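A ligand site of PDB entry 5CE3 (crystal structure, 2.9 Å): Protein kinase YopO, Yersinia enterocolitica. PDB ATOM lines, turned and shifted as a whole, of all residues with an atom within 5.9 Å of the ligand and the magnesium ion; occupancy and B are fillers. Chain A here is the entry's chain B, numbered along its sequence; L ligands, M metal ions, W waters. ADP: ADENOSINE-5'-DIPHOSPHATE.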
ATOM      1  N   LYS A  52     -10.732 -33.406  22.273  1.00  0.00           N
ATOM      2  CA  LYS A  52      -9.469 -33.418  21.564  1.00  0.00           C
ATOM      3  C   LYS A  52      -9.272 -32.073  20.886  1.00  0.00           C
ATOM      4  O   LYS A  52      -8.169 -31.735  20.462  1.00  0.00           O
ATOM      5  CB  LYS A  52      -9.517 -34.531  20.512  1.00  0.00           C
ATOM      6  CG  LYS A  52      -9.406 -35.901  21.163  1.00  0.00           C
ATOM      7  CD  LYS A  52      -9.761 -37.006  20.179  1.00  0.00           C
ATOM      8  CE  LYS A  52      -8.677 -37.205  19.130  1.00  0.00           C
ATOM      9  NZ  LYS A  52      -8.346 -38.633  18.839  1.00  0.00           N
ATOM     10  N   GLU A  57      -0.414 -33.543  23.095  1.00  0.00           N
ATOM     11  CA  GLU A  57      -1.725 -33.183  23.606  1.00  0.00           C
ATOM     12  C   GLU A  57      -1.935 -33.670  25.052  1.00  0.00           C
ATOM     13  O   GLU A  57      -1.229 -34.563  25.534  1.00  0.00           O
ATOM     14  CB  GLU A  57      -2.822 -33.758  22.701  1.00  0.00           C
ATOM     15  CG  GLU A  57      -2.752 -33.256  21.256  1.00  0.00           C
ATOM     16  CD  GLU A  57      -3.821 -33.836  20.329  1.00  0.00           C
ATOM     17  OE1 GLU A  57      -5.007 -33.904  20.736  1.00  0.00           O
ATOM     18  OE2 GLU A  57      -3.481 -34.201  19.182  1.00  0.00           O
ATOM     19  N   SER A  58      -2.889 -33.036  25.736  1.00  0.00           N
ATOM     20  CA  SER A  58      -3.401 -33.507  27.037  1.00  0.00           C
ATOM     21  C   SER A  58      -4.911 -33.510  26.963  1.00  0.00           C
ATOM     22  O   SER A  58      -5.466 -32.810  26.132  1.00  0.00           O
ATOM     23  CB  SER A  58      -2.924 -32.610  28.190  1.00  0.00           C
ATOM     24  OG  SER A  58      -3.225 -31.257  27.971  1.00  0.00           O
ATOM     25  N   ILE A  60      -8.633 -32.562  27.812  1.00  0.00           N
ATOM     26  CA  ILE A  60      -9.411 -31.453  28.385  1.00  0.00           C
ATOM     27  C   ILE A  60     -10.858 -31.910  28.479  1.00  0.00           C
ATOM     28  O   ILE A  60     -11.439 -32.307  27.470  1.00  0.00           O
ATOM     29  CB  ILE A  60      -9.344 -30.198  27.486  1.00  0.00           C
ATOM     30  CG1 ILE A  60      -8.087 -29.343  27.735  1.00  0.00           C
ATOM     31  CG2 ILE A  60     -10.572 -29.313  27.678  1.00  0.00           C
ATOM     32  CD1 ILE A  60      -6.776 -30.066  27.722  1.00  0.00           C
ATOM     33  N   VAL A  72     -13.491 -25.615  32.130  1.00  0.00           N
ATOM     34  CA  VAL A  72     -12.577 -26.560  31.519  1.00  0.00           C
ATOM     35  C   VAL A  72     -11.724 -27.142  32.624  1.00  0.00           C
ATOM     36  O   VAL A  72     -11.268 -26.421  33.514  1.00  0.00           O
ATOM     37  CB  VAL A  72     -11.698 -25.871  30.457  1.00  0.00           C
ATOM     38  CG1 VAL A  72     -10.412 -26.638  30.188  1.00  0.00           C
ATOM     39  CG2 VAL A  72     -12.488 -25.688  29.171  1.00  0.00           C
ATOM     40  N   LYS A  74      -8.296 -29.127  32.696  1.00  0.00           N
ATOM     41  CA  LYS A  74      -7.101 -29.610  32.046  1.00  0.00           C
ATOM     42  C   LYS A  74      -6.470 -30.721  32.888  1.00  0.00           C
ATOM     43  O   LYS A  74      -5.840 -30.421  33.892  1.00  0.00           O
ATOM     44  CB  LYS A  74      -6.129 -28.448  31.849  1.00  0.00           C
ATOM     45  CG  LYS A  74      -4.976 -28.744  30.914  1.00  0.00           C
ATOM     46  CD  LYS A  74      -4.013 -27.577  30.849  1.00  0.00           C
ATOM     47  CE  LYS A  74      -2.720 -27.973  30.162  1.00  0.00           C
ATOM     48  NZ  LYS A  74      -1.789 -26.826  29.970  1.00  0.00           N
ATOM     49  N   ARG A  77      -1.065 -35.066  32.342  1.00  0.00           N
ATOM     50  CA  ARG A  77      -0.505 -36.244  31.664  1.00  0.00           C
ATOM     51  C   ARG A  77      -0.154 -37.314  32.730  1.00  0.00           C
ATOM     52  O   ARG A  77       0.178 -36.978  33.878  1.00  0.00           O
ATOM     53  CB  ARG A  77       0.741 -35.882  30.841  1.00  0.00           C
ATOM     54  CG  ARG A  77       0.557 -34.658  29.877  1.00  0.00           C
ATOM     55  CD  ARG A  77       0.945 -34.908  28.412  1.00  0.00           C
ATOM     56  NE  ARG A  77       0.654 -33.834  27.452  1.00  0.00           N
ATOM     57  CZ  ARG A  77       1.179 -32.592  27.480  1.00  0.00           C
ATOM     58  NH1 ARG A  77       2.028 -32.190  28.424  1.00  0.00           N
ATOM     59  NH2 ARG A  77       0.825 -31.733  26.535  1.00  0.00           N
ATOM     60  N   GLU A  87       2.118 -24.653  36.299  1.00  0.00           N
ATOM     61  CA  GLU A  87       1.240 -23.796  35.493  1.00  0.00           C
ATOM     62  C   GLU A  87       0.269 -23.018  36.387  1.00  0.00           C
ATOM     63  O   GLU A  87       0.050 -21.835  36.166  1.00  0.00           O
ATOM     64  CB  GLU A  87       0.456 -24.621  34.441  1.00  0.00           C
ATOM     65  CG  GLU A  87      -0.298 -23.767  33.422  1.00  0.00           C
ATOM     66  CD  GLU A  87      -0.896 -24.554  32.239  1.00  0.00           C
ATOM     67  OE1 GLU A  87      -0.748 -25.807  32.191  1.00  0.00           O
ATOM     68  OE2 GLU A  87      -1.530 -23.900  31.369  1.00  0.00           O
ATOM     69  N   ALA A 105      -6.232 -16.455  30.333  1.00  0.00           N
ATOM     70  CA  ALA A 105      -7.154 -17.434  30.901  1.00  0.00           C
ATOM     71  C   ALA A 105      -7.480 -17.052  32.328  1.00  0.00           C
ATOM     72  O   ALA A 105      -6.641 -16.462  33.013  1.00  0.00           O
ATOM     73  CB  ALA A 105      -6.542 -18.822  30.894  1.00  0.00           C
ATOM     74  N   MET A 125     -10.517 -23.958  35.143  1.00  0.00           N
ATOM     75  CA  MET A 125     -10.580 -22.592  34.598  1.00  0.00           C
ATOM     76  C   MET A 125     -11.862 -22.351  33.776  1.00  0.00           C
ATOM     77  O   MET A 125     -12.570 -23.292  33.444  1.00  0.00           O
ATOM     78  CB  MET A 125      -9.365 -22.355  33.699  1.00  0.00           C
ATOM     79  CG  MET A 125      -9.342 -23.232  32.457  1.00  0.00           C
ATOM     80  SD  MET A 125      -7.903 -22.899  31.447  1.00  0.00           S
ATOM     81  CE  MET A 125      -6.899 -24.355  31.762  1.00  0.00           C
ATOM     82  N   ASP A 126     -12.133 -21.095  33.432  1.00  0.00           N
ATOM     83  CA  ASP A 126     -13.300 -20.744  32.619  1.00  0.00           C
ATOM     84  C   ASP A 126     -13.095 -21.206  31.181  1.00  0.00           C
ATOM     85  O   ASP A 126     -11.988 -21.122  30.648  1.00  0.00           O
ATOM     86  CB  ASP A 126     -13.555 -19.232  32.623  1.00  0.00           C
ATOM     87  CG  ASP A 126     -13.980 -18.695  33.983  1.00  0.00           C
ATOM     88  OD1 ASP A 126     -14.305 -19.467  34.902  1.00  0.00           O
ATOM     89  OD2 ASP A 126     -14.021 -17.471  34.156  1.00  0.00           O
ATOM     90  N   GLU A 127     -14.168 -21.675  30.546  1.00  0.00           N
ATOM     91  CA  GLU A 127     -14.116 -22.077  29.136  1.00  0.00           C
ATOM     92  C   GLU A 127     -14.153 -20.823  28.317  1.00  0.00           C
ATOM     93  O   GLU A 127     -15.021 -19.984  28.531  1.00  0.00           O
ATOM     94  CB  GLU A 127     -15.343 -22.938  28.764  1.00  0.00           C
ATOM     95  CG  GLU A 127     -15.391 -23.386  27.297  1.00  0.00           C
ATOM     96  CD  GLU A 127     -16.683 -24.090  26.906  1.00  0.00           C
ATOM     97  OE1 GLU A 127     -17.772 -23.565  27.189  1.00  0.00           O
ATOM     98  OE2 GLU A 127     -16.603 -25.165  26.262  1.00  0.00           O
ATOM     99  N   VAL A 128     -13.225 -20.691  27.383  1.00  0.00           N
ATOM    100  CA  VAL A 128     -13.336 -19.674  26.351  1.00  0.00           C
ATOM    101  C   VAL A 128     -14.181 -20.294  25.256  1.00  0.00           C
ATOM    102  O   VAL A 128     -13.690 -21.104  24.459  1.00  0.00           O
ATOM    103  CB  VAL A 128     -11.976 -19.213  25.811  1.00  0.00           C
ATOM    104  CG1 VAL A 128     -12.161 -18.072  24.824  1.00  0.00           C
ATOM    105  CG2 VAL A 128     -11.076 -18.765  26.957  1.00  0.00           C
ATOM    106  N   ASP A 129     -15.466 -19.950  25.251  1.00  0.00           N
ATOM    107  CA  ASP A 129     -16.425 -20.559  24.346  1.00  0.00           C
ATOM    108  C   ASP A 129     -16.304 -19.924  22.975  1.00  0.00           C
ATOM    109  O   ASP A 129     -16.761 -18.816  22.773  1.00  0.00           O
ATOM    110  CB  ASP A 129     -17.848 -20.407  24.886  1.00  0.00           C
ATOM    111  CG  ASP A 129     -18.901 -21.046  23.993  1.00  0.00           C
ATOM    112  OD1 ASP A 129     -18.605 -22.056  23.313  1.00  0.00           O
ATOM    113  OD2 ASP A 129     -20.036 -20.536  23.979  1.00  0.00           O
ATOM    114  N   ARG A 132     -10.412 -21.793  18.172  1.00  0.00           N
ATOM    115  CA  ARG A 132      -8.961 -21.591  18.353  1.00  0.00           C
ATOM    116  C   ARG A 132      -8.502 -20.596  17.291  1.00  0.00           C
ATOM    117  O   ARG A 132      -9.192 -20.362  16.304  1.00  0.00           O
ATOM    118  CB  ARG A 132      -8.178 -22.897  18.241  1.00  0.00           C
ATOM    119  CG  ARG A 132      -9.016 -24.131  18.563  1.00  0.00           C
ATOM    120  CD  ARG A 132      -8.206 -25.236  19.247  1.00  0.00           C
ATOM    121  NE  ARG A 132      -7.229 -25.908  18.413  1.00  0.00           N
ATOM    122  CZ  ARG A 132      -6.435 -26.886  18.844  1.00  0.00           C
ATOM    123  NH1 ARG A 132      -6.525 -27.335  20.094  1.00  0.00           N
ATOM    124  NH2 ARG A 132      -5.552 -27.425  18.027  1.00  0.00           N
ATOM    125  N   ASP A 181       5.423 -20.680  24.544  1.00  0.00           N
ATOM    126  CA  ASP A 181       4.688 -21.545  23.643  1.00  0.00           C
ATOM    127  C   ASP A 181       3.409 -20.861  23.112  1.00  0.00           C
ATOM    128  O   ASP A 181       2.379 -21.524  22.895  1.00  0.00           O
ATOM    129  CB  ASP A 181       4.382 -22.841  24.396  1.00  0.00           C
ATOM    130  CG  ASP A 181       4.006 -23.998  23.469  1.00  0.00           C
ATOM    131  OD1 ASP A 181       4.346 -23.965  22.265  1.00  0.00           O
ATOM    132  OD2 ASP A 181       3.335 -24.948  23.982  1.00  0.00           O
ATOM    133  N   LYS A 183       1.258 -19.905  20.296  1.00  0.00           N
ATOM    134  CA  LYS A 183       1.058 -20.437  18.941  1.00  0.00           C
ATOM    135  C   LYS A 183      -0.450 -20.586  18.720  1.00  0.00           C
ATOM    136  O   LYS A 183      -1.225 -20.440  19.665  1.00  0.00           O
ATOM    137  CB  LYS A 183       1.815 -21.757  18.762  1.00  0.00           C
ATOM    138  CG  LYS A 183       1.376 -22.903  19.655  1.00  0.00           C
ATOM    139  CD  LYS A 183       2.304 -24.085  19.418  1.00  0.00           C
ATOM    140  CE  LYS A 183       1.925 -25.283  20.259  1.00  0.00           C
ATOM    141  NZ  LYS A 183       2.628 -26.515  19.795  1.00  0.00           N
ATOM    142  N   GLY A 185      -2.682 -22.909  18.555  1.00  0.00           N
ATOM    143  CA  GLY A 185      -3.434 -23.790  19.452  1.00  0.00           C
ATOM    144  C   GLY A 185      -3.603 -23.254  20.860  1.00  0.00           C
ATOM    145  O   GLY A 185      -4.611 -23.546  21.534  1.00  0.00           O
ATOM    146  N   ASN A 186      -2.647 -22.429  21.301  1.00  0.00           N
ATOM    147  CA  ASN A 186      -2.694 -21.815  22.620  1.00  0.00           C
ATOM    148  C   ASN A 186      -3.320 -20.402  22.657  1.00  0.00           C
ATOM    149  O   ASN A 186      -3.108 -19.650  23.607  1.00  0.00           O
ATOM    150  CB  ASN A 186      -1.278 -21.852  23.199  1.00  0.00           C
ATOM    151  CG  ASN A 186      -0.778 -23.272  23.356  1.00  0.00           C
ATOM    152  OD1 ASN A 186      -1.570 -24.200  23.454  1.00  0.00           O
ATOM    153  ND2 ASN A 186       0.527 -23.446  23.374  1.00  0.00           N
ATOM    154  N   VAL A 188      -7.307 -18.833  21.999  1.00  0.00           N
ATOM    155  CA  VAL A 188      -8.695 -19.149  21.752  1.00  0.00           C
ATOM    156  C   VAL A 188      -9.517 -17.868  21.790  1.00  0.00           C
ATOM    157  O   VAL A 188      -9.362 -17.062  22.709  1.00  0.00           O
ATOM    158  CB  VAL A 188      -9.193 -20.141  22.818  1.00  0.00           C
ATOM    159  CG1 VAL A 188     -10.666 -20.515  22.604  1.00  0.00           C
ATOM    160  CG2 VAL A 188      -8.325 -21.394  22.804  1.00  0.00           C
ATOM    161  N   ILE A 199      -3.731 -19.087  26.597  1.00  0.00           N
ATOM    162  CA  ILE A 199      -3.815 -20.229  27.507  1.00  0.00           C
ATOM    163  C   ILE A 199      -2.500 -20.985  27.467  1.00  0.00           C
ATOM    164  O   ILE A 199      -1.574 -20.579  26.749  1.00  0.00           O
ATOM    165  CB  ILE A 199      -4.991 -21.148  27.105  1.00  0.00           C
ATOM    166  CG1 ILE A 199      -4.831 -21.656  25.665  1.00  0.00           C
ATOM    167  CG2 ILE A 199      -6.320 -20.411  27.239  1.00  0.00           C
ATOM    168  CD1 ILE A 199      -5.811 -22.753  25.302  1.00  0.00           C
ATOM    169  N   ASP A 200      -2.411 -22.081  28.205  1.00  0.00           N
ATOM    170  CA  ASP A 200      -1.283 -23.035  28.120  1.00  0.00           C
ATOM    171  C   ASP A 200       0.046 -22.400  28.565  1.00  0.00           C
ATOM    172  O   ASP A 200       0.965 -22.182  27.774  1.00  0.00           O
ATOM    173  CB  ASP A 200      -1.175 -23.647  26.695  1.00  0.00           C
ATOM    174  CG  ASP A 200      -0.355 -24.958  26.660  1.00  0.00           C
ATOM    175  OD1 ASP A 200       0.166 -25.400  27.713  1.00  0.00           O
ATOM    176  OD2 ASP A 200      -0.209 -25.570  25.574  1.00  0.00           O
ATOM    177  N   GLY A 202       2.028 -24.126  30.490  1.00  0.00           N
ATOM    178  CA  GLY A 202       2.701 -25.319  30.972  1.00  0.00           C
ATOM    179  C   GLY A 202       4.212 -25.256  30.848  1.00  0.00           C
ATOM    180  O   GLY A 202       4.920 -25.658  31.789  1.00  0.00           O
HETATM  181  PB  ADP L   1      -1.393 -28.641  26.159  1.00  0.00           P
HETATM  182  O1B ADP L   1      -1.543 -30.141  26.262  1.00  0.00           O
HETATM  183  O2B ADP L   1      -1.380 -28.121  24.738  1.00  0.00           O
HETATM  184  O3B ADP L   1      -0.271 -28.074  27.012  1.00  0.00           O
HETATM  185  PA  ADP L   1      -3.627 -26.812  26.466  1.00  0.00           P
HETATM  186  O1A ADP L   1      -3.812 -26.074  27.766  1.00  0.00           O
HETATM  187  O2A ADP L   1      -3.055 -26.073  25.277  1.00  0.00           O
HETATM  188  O3A ADP L   1      -2.791 -28.148  26.796  1.00  0.00           O
HETATM  189  O5' ADP L   1      -5.045 -27.419  26.007  1.00  0.00           O
HETATM  190  C5' ADP L   1      -5.235 -28.015  24.729  1.00  0.00           C
HETATM  191  C4' ADP L   1      -6.452 -27.448  24.001  1.00  0.00           C
HETATM  192  O4' ADP L   1      -7.565 -27.384  24.884  1.00  0.00           O
HETATM  193  C3' ADP L   1      -6.289 -26.036  23.452  1.00  0.00           C
HETATM  194  O3' ADP L   1      -5.779 -26.013  22.112  1.00  0.00           O
HETATM  195  C2' ADP L   1      -7.684 -25.461  23.506  1.00  0.00           C
HETATM  196  O2' ADP L   1      -8.452 -25.695  22.317  1.00  0.00           O
HETATM  197  C1' ADP L   1      -8.355 -26.218  24.616  1.00  0.00           C
HETATM  198  N9  ADP L   1      -8.465 -25.375  25.828  1.00  0.00           N
HETATM  199  C8  ADP L   1      -7.664 -25.318  26.909  1.00  0.00           C
HETATM  200  N7  ADP L   1      -8.135 -24.418  27.817  1.00  0.00           N
HETATM  201  C5  ADP L   1      -9.270 -23.899  27.298  1.00  0.00           C
HETATM  202  C6  ADP L   1     -10.287 -22.912  27.713  1.00  0.00           C
HETATM  203  N6  ADP L   1     -10.199 -22.265  28.896  1.00  0.00           N
HETATM  204  N1  ADP L   1     -11.310 -22.673  26.847  1.00  0.00           N
HETATM  205  C2  ADP L   1     -11.426 -23.298  25.655  1.00  0.00           C
HETATM  206  N3  ADP L   1     -10.533 -24.202  25.223  1.00  0.00           N
HETATM  207  C4  ADP L   1      -9.468 -24.537  25.994  1.00  0.00           C
HETATM  208 MG    MG M   1      -1.593 -26.326  23.986  1.00  0.00          MG
HETATM  209  O   HOH W   1       2.303 -26.477  26.558  1.00  0.00           O
HETATM  210  O   HOH W   2       0.273 -26.433  22.756  1.00  0.00           O
HETATM  211  O   HOH W   3      -3.008 -26.464  22.293  1.00  0.00           O
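NH1 of Arg 132 sits at hydrogen-bond distance from O3' of the ligand (2.5 Å). An oxygen (O3') of the ligand sits at hydrogen-bond distance from the backbone carbonyl oxygen (O) of Gly 185 (2.8 Å). An oxygen (O1A) of the ligand is in salt-bridge range of the side-chain amino group (NZ) of Lys 74. N of Val 128 sits at hydrogen-bond distance from N1 of the ligand, 2.8 Å away. N of Ser 58 lies within hydrogen-bond range of O1B of the ligand (3.2 Å). An oxygen (O1B) of the ligand lies within salt-bridge range of the guanidinium group (NH2) of Arg 77 (2.9 Å). A nitrogen (N6) of the ligand lies within hydrogen-bond range of the side-chain sulfur of Met 125, 3.5 Å away. O1B of the ligand is in hydrogen-bond range of OG of Ser 58 (2.6 Å). The backbone carbonyl oxygen (O) of Asp 126 sits at hydrogen-bond distance from a nitrogen (N6) of the ligand, 2.8 Å away.
NE of Arg 77 lies within hydrogen-bond range of O of Glu 57, at 2.8 Å. N of Val 72 sits at hydrogen-bond distance from O of Met 125, 2.8 Å away. ND2 of Asn 186 is in hydrogen-bond range of O of Asp 181 (2.7 Å). OD1 of Asp 200 is in salt-bridge range of NZ of Lys 74 (3.3 Å). NZ of Lys 74 is in salt-bridge range of OE1 of Glu 87 (2.7 Å). The backbone carbonyl oxygen (O) of Asn 186 sits at hydrogen-bond distance from the backbone NH (N) of Ile 199.
Residues that only touch the ligand: Ile 60 (3.5 Å), Ile 199 (3.5 Å), Glu 127 (3.7 Å), Glu 57 (3.8 Å) and Val 72 (3.8 Å). Hydrophobic or aromatic side chains within 4 Å of the ligand: Ile 60, Val 72, Met 125, Val 128 and Ile 199. Within 4 Å of the ligand: Glu 57, Ser 58, Ile 60, Val 72, Lys 74, Arg 77, Met 125, Asp 126, Glu 127, Val 128, Arg 132, Gly 185, Asn 186, Ile 199 and Asp 200. The nearest printed residue that does not touch the ligand is Val 188 (4.2 Å).
Within 4 Å of the magnesium ion: Asn 186 and Asp 200. The nearest printed residue that does not touch the magnesium ion is Gly 185 (4.8 Å).
O2B of the ligand binds the magnesium ion, at 2.0 Å. An oxygen (O2A) of the ligand binds the magnesium ion, 2.0 Å away. The side-chain amide oxygen (OD1) of Asn 186 binds the magnesium ion (2.2 Å). The magnesium ion is bound by water W3 (2.2 Å). Water W2 is bound to the magnesium ion (2.2 Å). The magnesium ion is bound by the side-chain carboxylate (OD2) of Asp 200, at 2.2 Å. The magnesium ion has six donor atoms within binding distance.
Water W3 lies within hydrogen-bond range of an oxygen (O3') of the ligand and the backbone carbonyl oxygen (O) of Gly 185. Water W1 lies within hydrogen-bond range of OD1 of Asp 200 (2.7 Å), O3B of the ligand (3.1 Å) and OD2 of Asp 181 (3.2 Å).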
